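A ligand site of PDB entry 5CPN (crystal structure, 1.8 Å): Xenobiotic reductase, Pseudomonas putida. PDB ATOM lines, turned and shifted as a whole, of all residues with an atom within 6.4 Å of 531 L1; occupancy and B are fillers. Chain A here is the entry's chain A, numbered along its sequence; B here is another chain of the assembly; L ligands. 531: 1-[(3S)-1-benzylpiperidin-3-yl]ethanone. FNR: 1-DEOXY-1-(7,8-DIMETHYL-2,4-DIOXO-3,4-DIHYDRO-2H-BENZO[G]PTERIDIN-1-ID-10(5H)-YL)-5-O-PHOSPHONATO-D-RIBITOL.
An oxygen (O15) of 531 L1 lies close to a nitrogen (N1) of FNR L2.
ND1 of His 181 lies within hydrogen-bond range of O15 of 531 L1 (2.7 Å).
An oxygen (O15) of 531 L1 is in hydrogen-bond range of a ring nitrogen (NE2) of His 178, 2.9 Å away.
An oxygen (O2) of FNR L2 is in hydrogen-bond range of a ring nitrogen (NE2) of His 178.
The backbone NH of Trp 302 is in hydrogen-bond range of an oxygen (O5') of FNR L2.
O2P of FNR L2 lies within hydrogen-bond range of N of Arg 326.
NE of Arg 326 lies within salt-bridge range of O2P of FNR L2, 2.9 Å away.
The backbone NH of Cys 25 is in hydrogen-bond range of an oxygen (O4) of FNR L2.
An oxygen (O4) of FNR L2 sits at hydrogen-bond distance from the side-chain sulfur (SG) of Cys 25 (3.3 Å).
An oxygen (O4) of FNR L2 sits at hydrogen-bond distance from the backbone NH (N) of Ala 57, at 3.1 Å.
The side-chain amide oxygen of Gln 99 lies within hydrogen-bond range of a nitrogen (N3) of FNR L2, 2.7 Å away.
The guanidinium group of Arg 231 sits at hydrogen-bond distance from an oxygen (O2') of FNR L2 (2.9 Å).
The backbone carbonyl oxygen (O) of Pro 23 sits close to an oxygen (O2') of FNR L2 (2.9 Å).
A ring nitrogen (ND1) of His 178 lies close to the backbone NH (N) of Ala 180, 3.3 Å away.
Merely in contact with 531 L1: Tyr 27 (3.2 Å), Ile 66 (3.4 Å), Tyr 183 (3.2 Å), Trp 302 (3.7 Å), Arg 326 (3.99 Å) and Trp 358 of chain B (3.8 Å).
Hydrophobic or aromatic side chains within 4 Å of 531 L1: Ile 66, His 178, His 181, Tyr 183, Trp 302 and Trp 358 of chain B.
Of the 17 residues printed, 8 come within 4 Å of 531 L1.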
ATOM      1  N   PRO A  23     -21.585  30.300   7.307  1.00  0.00           N
ATOM      2  CA  PRO A  23     -21.084  29.183   6.527  1.00  0.00           C
ATOM      3  C   PRO A  23     -20.106  28.313   7.287  1.00  0.00           C
ATOM      4  O   PRO A  23     -19.165  28.824   7.879  1.00  0.00           O
ATOM      5  CB  PRO A  23     -20.402  29.878   5.341  1.00  0.00           C
ATOM      6  CG  PRO A  23     -20.051  31.212   5.843  1.00  0.00           C
ATOM      7  CD  PRO A  23     -21.137  31.592   6.792  1.00  0.00           C
ATOM      8  N   CYS A  25     -18.083  24.806   6.347  1.00  0.00           N
ATOM      9  CA  CYS A  25     -17.555  23.645   5.597  1.00  0.00           C
ATOM     10  C   CYS A  25     -17.794  22.319   6.290  1.00  0.00           C
ATOM     11  O   CYS A  25     -17.509  22.163   7.485  1.00  0.00           O
ATOM     12  CB  CYS A  25     -16.050  23.824   5.374  1.00  0.00           C
ATOM     13  SG  CYS A  25     -15.666  25.038   4.111  1.00  0.00           S
ATOM     14  N   TYR A  27     -16.805  19.317   4.520  1.00  0.00           N
ATOM     15  CA  TYR A  27     -15.773  18.473   3.942  1.00  0.00           C
ATOM     16  C   TYR A  27     -16.343  17.111   3.578  1.00  0.00           C
ATOM     17  O   TYR A  27     -15.654  16.094   3.700  1.00  0.00           O
ATOM     18  CB  TYR A  27     -14.580  18.307   4.909  1.00  0.00           C
ATOM     19  CG  TYR A  27     -14.073  19.623   5.455  1.00  0.00           C
ATOM     20  CD1 TYR A  27     -13.083  20.334   4.784  1.00  0.00           C
ATOM     21  CD2 TYR A  27     -14.598  20.155   6.616  1.00  0.00           C
ATOM     22  CE1 TYR A  27     -12.634  21.530   5.281  1.00  0.00           C
ATOM     23  CE2 TYR A  27     -14.142  21.372   7.116  1.00  0.00           C
ATOM     24  CZ  TYR A  27     -13.153  22.049   6.445  1.00  0.00           C
ATOM     25  OH  TYR A  27     -12.689  23.263   6.913  1.00  0.00           O
ATOM     26  N   ALA A  57     -18.714  27.560   2.405  1.00  0.00           N
ATOM     27  CA  ALA A  57     -17.822  28.002   1.356  1.00  0.00           C
ATOM     28  C   ALA A  57     -17.822  27.051   0.184  1.00  0.00           C
ATOM     29  O   ALA A  57     -17.405  25.887   0.278  1.00  0.00           O
ATOM     30  CB  ALA A  57     -16.401  28.176   1.908  1.00  0.00           C
ATOM     31  N   ILE A  66     -10.706  24.212  -0.660  1.00  0.00           N
ATOM     32  CA  ILE A  66      -9.697  24.005   0.380  1.00  0.00           C
ATOM     33  C   ILE A  66      -9.197  22.544   0.328  1.00  0.00           C
ATOM     34  O   ILE A  66      -7.988  22.285   0.337  1.00  0.00           O
ATOM     35  CB  ILE A  66     -10.258  24.302   1.787  1.00  0.00           C
ATOM     36  CG1 ILE A  66     -10.951  25.653   1.809  1.00  0.00           C
ATOM     37  CG2 ILE A  66      -9.161  24.247   2.778  1.00  0.00           C
ATOM     38  CD1 ILE A  66     -11.900  25.863   2.956  1.00  0.00           C
ATOM     39  N   GLN A  99     -22.234  31.061   0.471  1.00  0.00           N
ATOM     40  CA  GLN A  99     -20.949  31.734   0.430  1.00  0.00           C
ATOM     41  C   GLN A  99     -20.162  31.159  -0.740  1.00  0.00           C
ATOM     42  O   GLN A  99     -19.953  29.945  -0.777  1.00  0.00           O
ATOM     43  CB  GLN A  99     -20.167  31.521   1.720  1.00  0.00           C
ATOM     44  CG  GLN A  99     -18.854  32.261   1.739  1.00  0.00           C
ATOM     45  CD  GLN A  99     -18.032  31.964   2.964  1.00  0.00           C
ATOM     46  OE1 GLN A  99     -17.585  30.840   3.167  1.00  0.00           O
ATOM     47  NE2 GLN A  99     -17.851  32.980   3.812  1.00  0.00           N
ATOM     48  N   PRO A 112      -9.849  18.562   8.009  1.00  0.00           N
ATOM     49  CA  PRO A 112      -9.313  18.933   9.332  1.00  0.00           C
ATOM     50  C   PRO A 112      -9.023  17.758  10.263  1.00  0.00           C
ATOM     51  O   PRO A 112      -8.082  17.877  11.079  1.00  0.00           O
ATOM     52  CB  PRO A 112     -10.425  19.825   9.898  1.00  0.00           C
ATOM     53  CG  PRO A 112     -11.035  20.454   8.655  1.00  0.00           C
ATOM     54  CD  PRO A 112     -11.078  19.310   7.686  1.00  0.00           C
ATOM     55  N   HIS A 178     -16.651  35.403  -0.221  1.00  0.00           N
ATOM     56  CA  HIS A 178     -15.692  35.063   0.836  1.00  0.00           C
ATOM     57  C   HIS A 178     -14.385  35.821   0.586  1.00  0.00           C
ATOM     58  O   HIS A 178     -13.474  35.347  -0.116  1.00  0.00           O
ATOM     59  CB  HIS A 178     -15.444  33.547   0.905  1.00  0.00           C
ATOM     60  CG  HIS A 178     -14.852  33.088   2.195  1.00  0.00           C
ATOM     61  ND1 HIS A 178     -14.384  33.971   3.153  1.00  0.00           N
ATOM     62  CD2 HIS A 178     -14.696  31.836   2.716  1.00  0.00           C
ATOM     63  CE1 HIS A 178     -13.934  33.283   4.196  1.00  0.00           C
ATOM     64  NE2 HIS A 178     -14.120  31.985   3.963  1.00  0.00           N
ATOM     65  N   ALA A 180     -12.515  36.726   3.181  1.00  0.00           N
ATOM     66  CA  ALA A 180     -11.901  36.686   4.500  1.00  0.00           C
ATOM     67  C   ALA A 180     -11.024  35.448   4.732  1.00  0.00           C
ATOM     68  O   ALA A 180     -10.859  34.611   3.858  1.00  0.00           O
ATOM     69  CB  ALA A 180     -12.988  36.765   5.582  1.00  0.00           C
ATOM     70  N   HIS A 181     -10.440  35.374   5.928  1.00  0.00           N
ATOM     71  CA  HIS A 181      -9.822  34.149   6.462  1.00  0.00           C
ATOM     72  C   HIS A 181      -8.628  33.644   5.649  1.00  0.00           C
ATOM     73  O   HIS A 181      -8.264  32.483   5.729  1.00  0.00           O
ATOM     74  CB  HIS A 181     -10.863  33.010   6.583  1.00  0.00           C
ATOM     75  CG  HIS A 181     -12.042  33.381   7.444  1.00  0.00           C
ATOM     76  ND1 HIS A 181     -13.199  32.622   7.469  1.00  0.00           N
ATOM     77  CD2 HIS A 181     -12.243  34.404   8.299  1.00  0.00           C
ATOM     78  CE1 HIS A 181     -14.062  33.180   8.297  1.00  0.00           C
ATOM     79  NE2 HIS A 181     -13.498  34.254   8.822  1.00  0.00           N
ATOM     80  N   TYR A 183      -7.932  33.556   2.435  1.00  0.00           N
ATOM     81  CA  TYR A 183      -8.120  32.886   1.135  1.00  0.00           C
ATOM     82  C   TYR A 183      -7.868  33.930   0.049  1.00  0.00           C
ATOM     83  O   TYR A 183      -7.304  34.976   0.340  1.00  0.00           O
ATOM     84  CB  TYR A 183      -9.505  32.240   1.089  1.00  0.00           C
ATOM     85  CG  TYR A 183      -9.718  31.186   2.191  1.00  0.00           C
ATOM     86  CD1 TYR A 183      -8.915  30.027   2.253  1.00  0.00           C
ATOM     87  CD2 TYR A 183     -10.705  31.346   3.159  1.00  0.00           C
ATOM     88  CE1 TYR A 183      -9.088  29.060   3.259  1.00  0.00           C
ATOM     89  CE2 TYR A 183     -10.886  30.385   4.176  1.00  0.00           C
ATOM     90  CZ  TYR A 183     -10.070  29.234   4.211  1.00  0.00           C
ATOM     91  OH  TYR A 183     -10.236  28.260   5.208  1.00  0.00           O
ATOM     92  N   ARG A 231     -17.922  38.658   3.305  1.00  0.00           N
ATOM     93  CA  ARG A 231     -17.203  38.481   4.542  1.00  0.00           C
ATOM     94  C   ARG A 231     -15.765  38.936   4.299  1.00  0.00           C
ATOM     95  O   ARG A 231     -15.162  38.622   3.260  1.00  0.00           O
ATOM     96  CB  ARG A 231     -17.257  37.019   5.044  1.00  0.00           C
ATOM     97  CG  ARG A 231     -16.407  36.816   6.310  1.00  0.00           C
ATOM     98  CD  ARG A 231     -17.191  36.466   7.536  1.00  0.00           C
ATOM     99  NE  ARG A 231     -17.213  35.044   7.716  1.00  0.00           N
ATOM    100  CZ  ARG A 231     -17.516  34.367   8.836  1.00  0.00           C
ATOM    101  NH1 ARG A 231     -17.761  34.898  10.026  1.00  0.00           N
ATOM    102  NH2 ARG A 231     -17.509  33.081   8.736  1.00  0.00           N
ATOM    103  N   PHE A 269      -6.828  36.054   9.324  1.00  0.00           N
ATOM    104  CA  PHE A 269      -6.090  34.794   9.289  1.00  0.00           C
ATOM    105  C   PHE A 269      -5.110  34.697   8.113  1.00  0.00           C
ATOM    106  O   PHE A 269      -4.912  33.599   7.577  1.00  0.00           O
ATOM    107  CB  PHE A 269      -7.041  33.579   9.196  1.00  0.00           C
ATOM    108  CG  PHE A 269      -8.002  33.448  10.353  1.00  0.00           C
ATOM    109  CD1 PHE A 269      -7.537  33.356  11.658  1.00  0.00           C
ATOM    110  CD2 PHE A 269      -9.366  33.383  10.128  1.00  0.00           C
ATOM    111  CE1 PHE A 269      -8.414  33.230  12.726  1.00  0.00           C
ATOM    112  CE2 PHE A 269     -10.258  33.249  11.190  1.00  0.00           C
ATOM    113  CZ  PHE A 269      -9.786  33.174  12.489  1.00  0.00           C
ATOM    114  N   TRP A 278      -8.902  35.295  21.441  1.00  0.00           N
ATOM    115  CA  TRP A 278     -10.137  34.525  21.514  1.00  0.00           C
ATOM    116  C   TRP A 278     -10.856  34.726  22.838  1.00  0.00           C
ATOM    117  O   TRP A 278     -10.229  34.722  23.901  1.00  0.00           O
ATOM    118  CB  TRP A 278      -9.844  33.044  21.322  1.00  0.00           C
ATOM    119  CG  TRP A 278      -9.066  32.736  20.073  1.00  0.00           C
ATOM    120  CD1 TRP A 278      -7.763  32.343  19.992  1.00  0.00           C
ATOM    121  CD2 TRP A 278      -9.557  32.791  18.730  1.00  0.00           C
ATOM    122  NE1 TRP A 278      -7.406  32.145  18.683  1.00  0.00           N
ATOM    123  CE2 TRP A 278      -8.491  32.402  17.893  1.00  0.00           C
ATOM    124  CE3 TRP A 278     -10.793  33.104  18.159  1.00  0.00           C
ATOM    125  CZ2 TRP A 278      -8.630  32.346  16.505  1.00  0.00           C
ATOM    126  CZ3 TRP A 278     -10.923  33.041  16.794  1.00  0.00           C
ATOM    127  CH2 TRP A 278      -9.851  32.667  15.972  1.00  0.00           C
ATOM    128  N   TRP A 302     -17.804  34.049  16.324  1.00  0.00           N
ATOM    129  CA  TRP A 302     -16.621  33.765  17.138  1.00  0.00           C
ATOM    130  C   TRP A 302     -16.883  34.022  18.614  1.00  0.00           C
ATOM    131  O   TRP A 302     -16.165  34.814  19.232  1.00  0.00           O
ATOM    132  CB  TRP A 302     -15.407  34.612  16.697  1.00  0.00           C
ATOM    133  CG  TRP A 302     -15.105  34.572  15.212  1.00  0.00           C
ATOM    134  CD1 TRP A 302     -15.354  35.546  14.292  1.00  0.00           C
ATOM    135  CD2 TRP A 302     -14.490  33.494  14.497  1.00  0.00           C
ATOM    136  NE1 TRP A 302     -14.928  35.156  13.051  1.00  0.00           N
ATOM    137  CE2 TRP A 302     -14.402  33.886  13.149  1.00  0.00           C
ATOM    138  CE3 TRP A 302     -14.011  32.236  14.862  1.00  0.00           C
ATOM    139  CZ2 TRP A 302     -13.865  33.082  12.184  1.00  0.00           C
ATOM    140  CZ3 TRP A 302     -13.461  31.438  13.893  1.00  0.00           C
ATOM    141  CH2 TRP A 302     -13.393  31.858  12.572  1.00  0.00           C
ATOM    142  N   ARG A 326     -20.849  26.949  15.682  1.00  0.00           N
ATOM    143  CA  ARG A 326     -20.600  25.697  16.358  1.00  0.00           C
ATOM    144  C   ARG A 326     -21.746  25.277  17.273  1.00  0.00           C
ATOM    145  O   ARG A 326     -22.018  24.078  17.383  1.00  0.00           O
ATOM    146  CB  ARG A 326     -19.283  25.770  17.117  1.00  0.00           C
ATOM    147  CG  ARG A 326     -18.081  25.634  16.181  1.00  0.00           C
ATOM    148  CD  ARG A 326     -16.763  25.916  16.866  1.00  0.00           C
ATOM    149  NE  ARG A 326     -16.666  27.333  17.215  1.00  0.00           N
ATOM    150  CZ  ARG A 326     -15.570  27.926  17.694  1.00  0.00           C
ATOM    151  NH1 ARG A 326     -14.453  27.243  17.835  1.00  0.00           N
ATOM    152  NH2 ARG A 326     -15.618  29.219  18.020  1.00  0.00           N
ATOM    153  N   TRP B 358     -14.777  19.624  15.430  1.00  0.00           N
ATOM    154  CA  TRP B 358     -14.859  20.988  15.825  1.00  0.00           C
ATOM    155  C   TRP B 358     -15.336  21.138  17.252  1.00  0.00           C
ATOM    156  O   TRP B 358     -14.979  22.102  17.918  1.00  0.00           O
ATOM    157  CB  TRP B 358     -15.773  21.717  14.833  1.00  0.00           C
ATOM    158  CG  TRP B 358     -15.192  21.667  13.443  1.00  0.00           C
ATOM    159  CD1 TRP B 358     -15.544  20.817  12.414  1.00  0.00           C
ATOM    160  CD2 TRP B 358     -14.088  22.427  12.961  1.00  0.00           C
ATOM    161  NE1 TRP B 358     -14.745  21.050  11.316  1.00  0.00           N
ATOM    162  CE2 TRP B 358     -13.854  22.052  11.631  1.00  0.00           C
ATOM    163  CE3 TRP B 358     -13.308  23.446  13.521  1.00  0.00           C
ATOM    164  CZ2 TRP B 358     -12.850  22.643  10.857  1.00  0.00           C
ATOM    165  CZ3 TRP B 358     -12.326  24.038  12.729  1.00  0.00           C
ATOM    166  CH2 TRP B 358     -12.105  23.624  11.434  1.00  0.00           C
HETATM  167  C1  531 L   1     -11.502  29.052  10.417  1.00  0.00           C
HETATM  168  C2  531 L   1     -11.750  28.620  11.867  1.00  0.00           C
HETATM  169  C3  531 L   1     -10.808  28.759  12.771  1.00  0.00           C
HETATM  170  C4  531 L   1     -11.068  28.322  14.224  1.00  0.00           C
HETATM  171  C5  531 L   1     -12.242  27.818  14.567  1.00  0.00           C
HETATM  172  C6  531 L   1     -13.331  27.646  13.516  1.00  0.00           C
HETATM  173  C7  531 L   1     -13.106  28.023  12.266  1.00  0.00           C
HETATM  174  N8  531 L   1     -12.154  28.297   9.503  1.00  0.00           N
HETATM  175  C9  531 L   1     -12.165  28.839   8.285  1.00  0.00           C
HETATM  176  C10 531 L   1     -13.146  28.149   7.373  1.00  0.00           C
HETATM  177  C11 531 L   1     -12.609  26.764   7.038  1.00  0.00           C
HETATM  178  C12 531 L   1     -12.132  26.088   8.327  1.00  0.00           C
HETATM  179  C13 531 L   1     -11.696  27.035   9.461  1.00  0.00           C
HETATM  180  C14 531 L   1     -13.629  28.943   6.123  1.00  0.00           C
HETATM  181  O15 531 L   1     -13.405  30.306   6.172  1.00  0.00           O
HETATM  182  C16 531 L   1     -13.393  28.296   4.757  1.00  0.00           C
HETATM  183  C9A FNR L   2     -16.043  27.517   9.945  1.00  0.00           C
HETATM  184  N10 FNR L   2     -16.172  28.939   9.548  1.00  0.00           N
HETATM  185  CAA FNR L   2     -16.378  29.328   8.142  1.00  0.00           C
HETATM  186  N1  FNR L   2     -16.110  30.580   7.742  1.00  0.00           N
HETATM  187  C2  FNR L   2     -16.458  30.916   6.482  1.00  0.00           C
HETATM  188  O2  FNR L   2     -16.431  32.065   6.141  1.00  0.00           O
HETATM  189  N3  FNR L   2     -16.822  29.936   5.578  1.00  0.00           N
HETATM  190  C4  FNR L   2     -16.864  28.664   5.906  1.00  0.00           C
HETATM  191  O4  FNR L   2     -17.210  27.830   5.082  1.00  0.00           O
HETATM  192  C4A FNR L   2     -16.466  28.344   7.196  1.00  0.00           C
HETATM  193  N5  FNR L   2     -16.306  26.951   7.580  1.00  0.00           N
HETATM  194  C5A FNR L   2     -16.100  26.535   8.972  1.00  0.00           C
HETATM  195  C6  FNR L   2     -16.416  25.222   9.282  1.00  0.00           C
HETATM  196  C7  FNR L   2     -16.593  24.877  10.609  1.00  0.00           C
HETATM  197  C7M FNR L   2     -16.972  23.436  10.872  1.00  0.00           C
HETATM  198  C8  FNR L   2     -16.425  25.814  11.599  1.00  0.00           C
HETATM  199  C8M FNR L   2     -16.648  25.393  13.041  1.00  0.00           C
HETATM  200  C9  FNR L   2     -16.104  27.108  11.305  1.00  0.00           C
HETATM  201  C1' FNR L   2     -16.160  30.026  10.549  1.00  0.00           C
HETATM  202  C2' FNR L   2     -17.593  30.137  11.086  1.00  0.00           C
HETATM  203  O2' FNR L   2     -18.369  30.671  10.036  1.00  0.00           O
HETATM  204  C3' FNR L   2     -17.688  30.993  12.365  1.00  0.00           C
HETATM  205  O3' FNR L   2     -17.132  32.289  12.064  1.00  0.00           O
HETATM  206  C4' FNR L   2     -16.942  30.339  13.520  1.00  0.00           C
HETATM  207  O4' FNR L   2     -17.387  29.014  13.696  1.00  0.00           O
HETATM  208  C5' FNR L   2     -17.129  31.088  14.846  1.00  0.00           C
HETATM  209  O5' FNR L   2     -18.475  31.229  15.180  1.00  0.00           O
HETATM  210  P   FNR L   2     -18.995  30.331  16.434  1.00  0.00           P
HETATM  211  O1P FNR L   2     -18.136  30.670  17.619  1.00  0.00           O
HETATM  212  O2P FNR L   2     -18.788  28.885  15.970  1.00  0.00           O
HETATM  213  O3P FNR L   2     -20.457  30.651  16.711  1.00  0.00           O
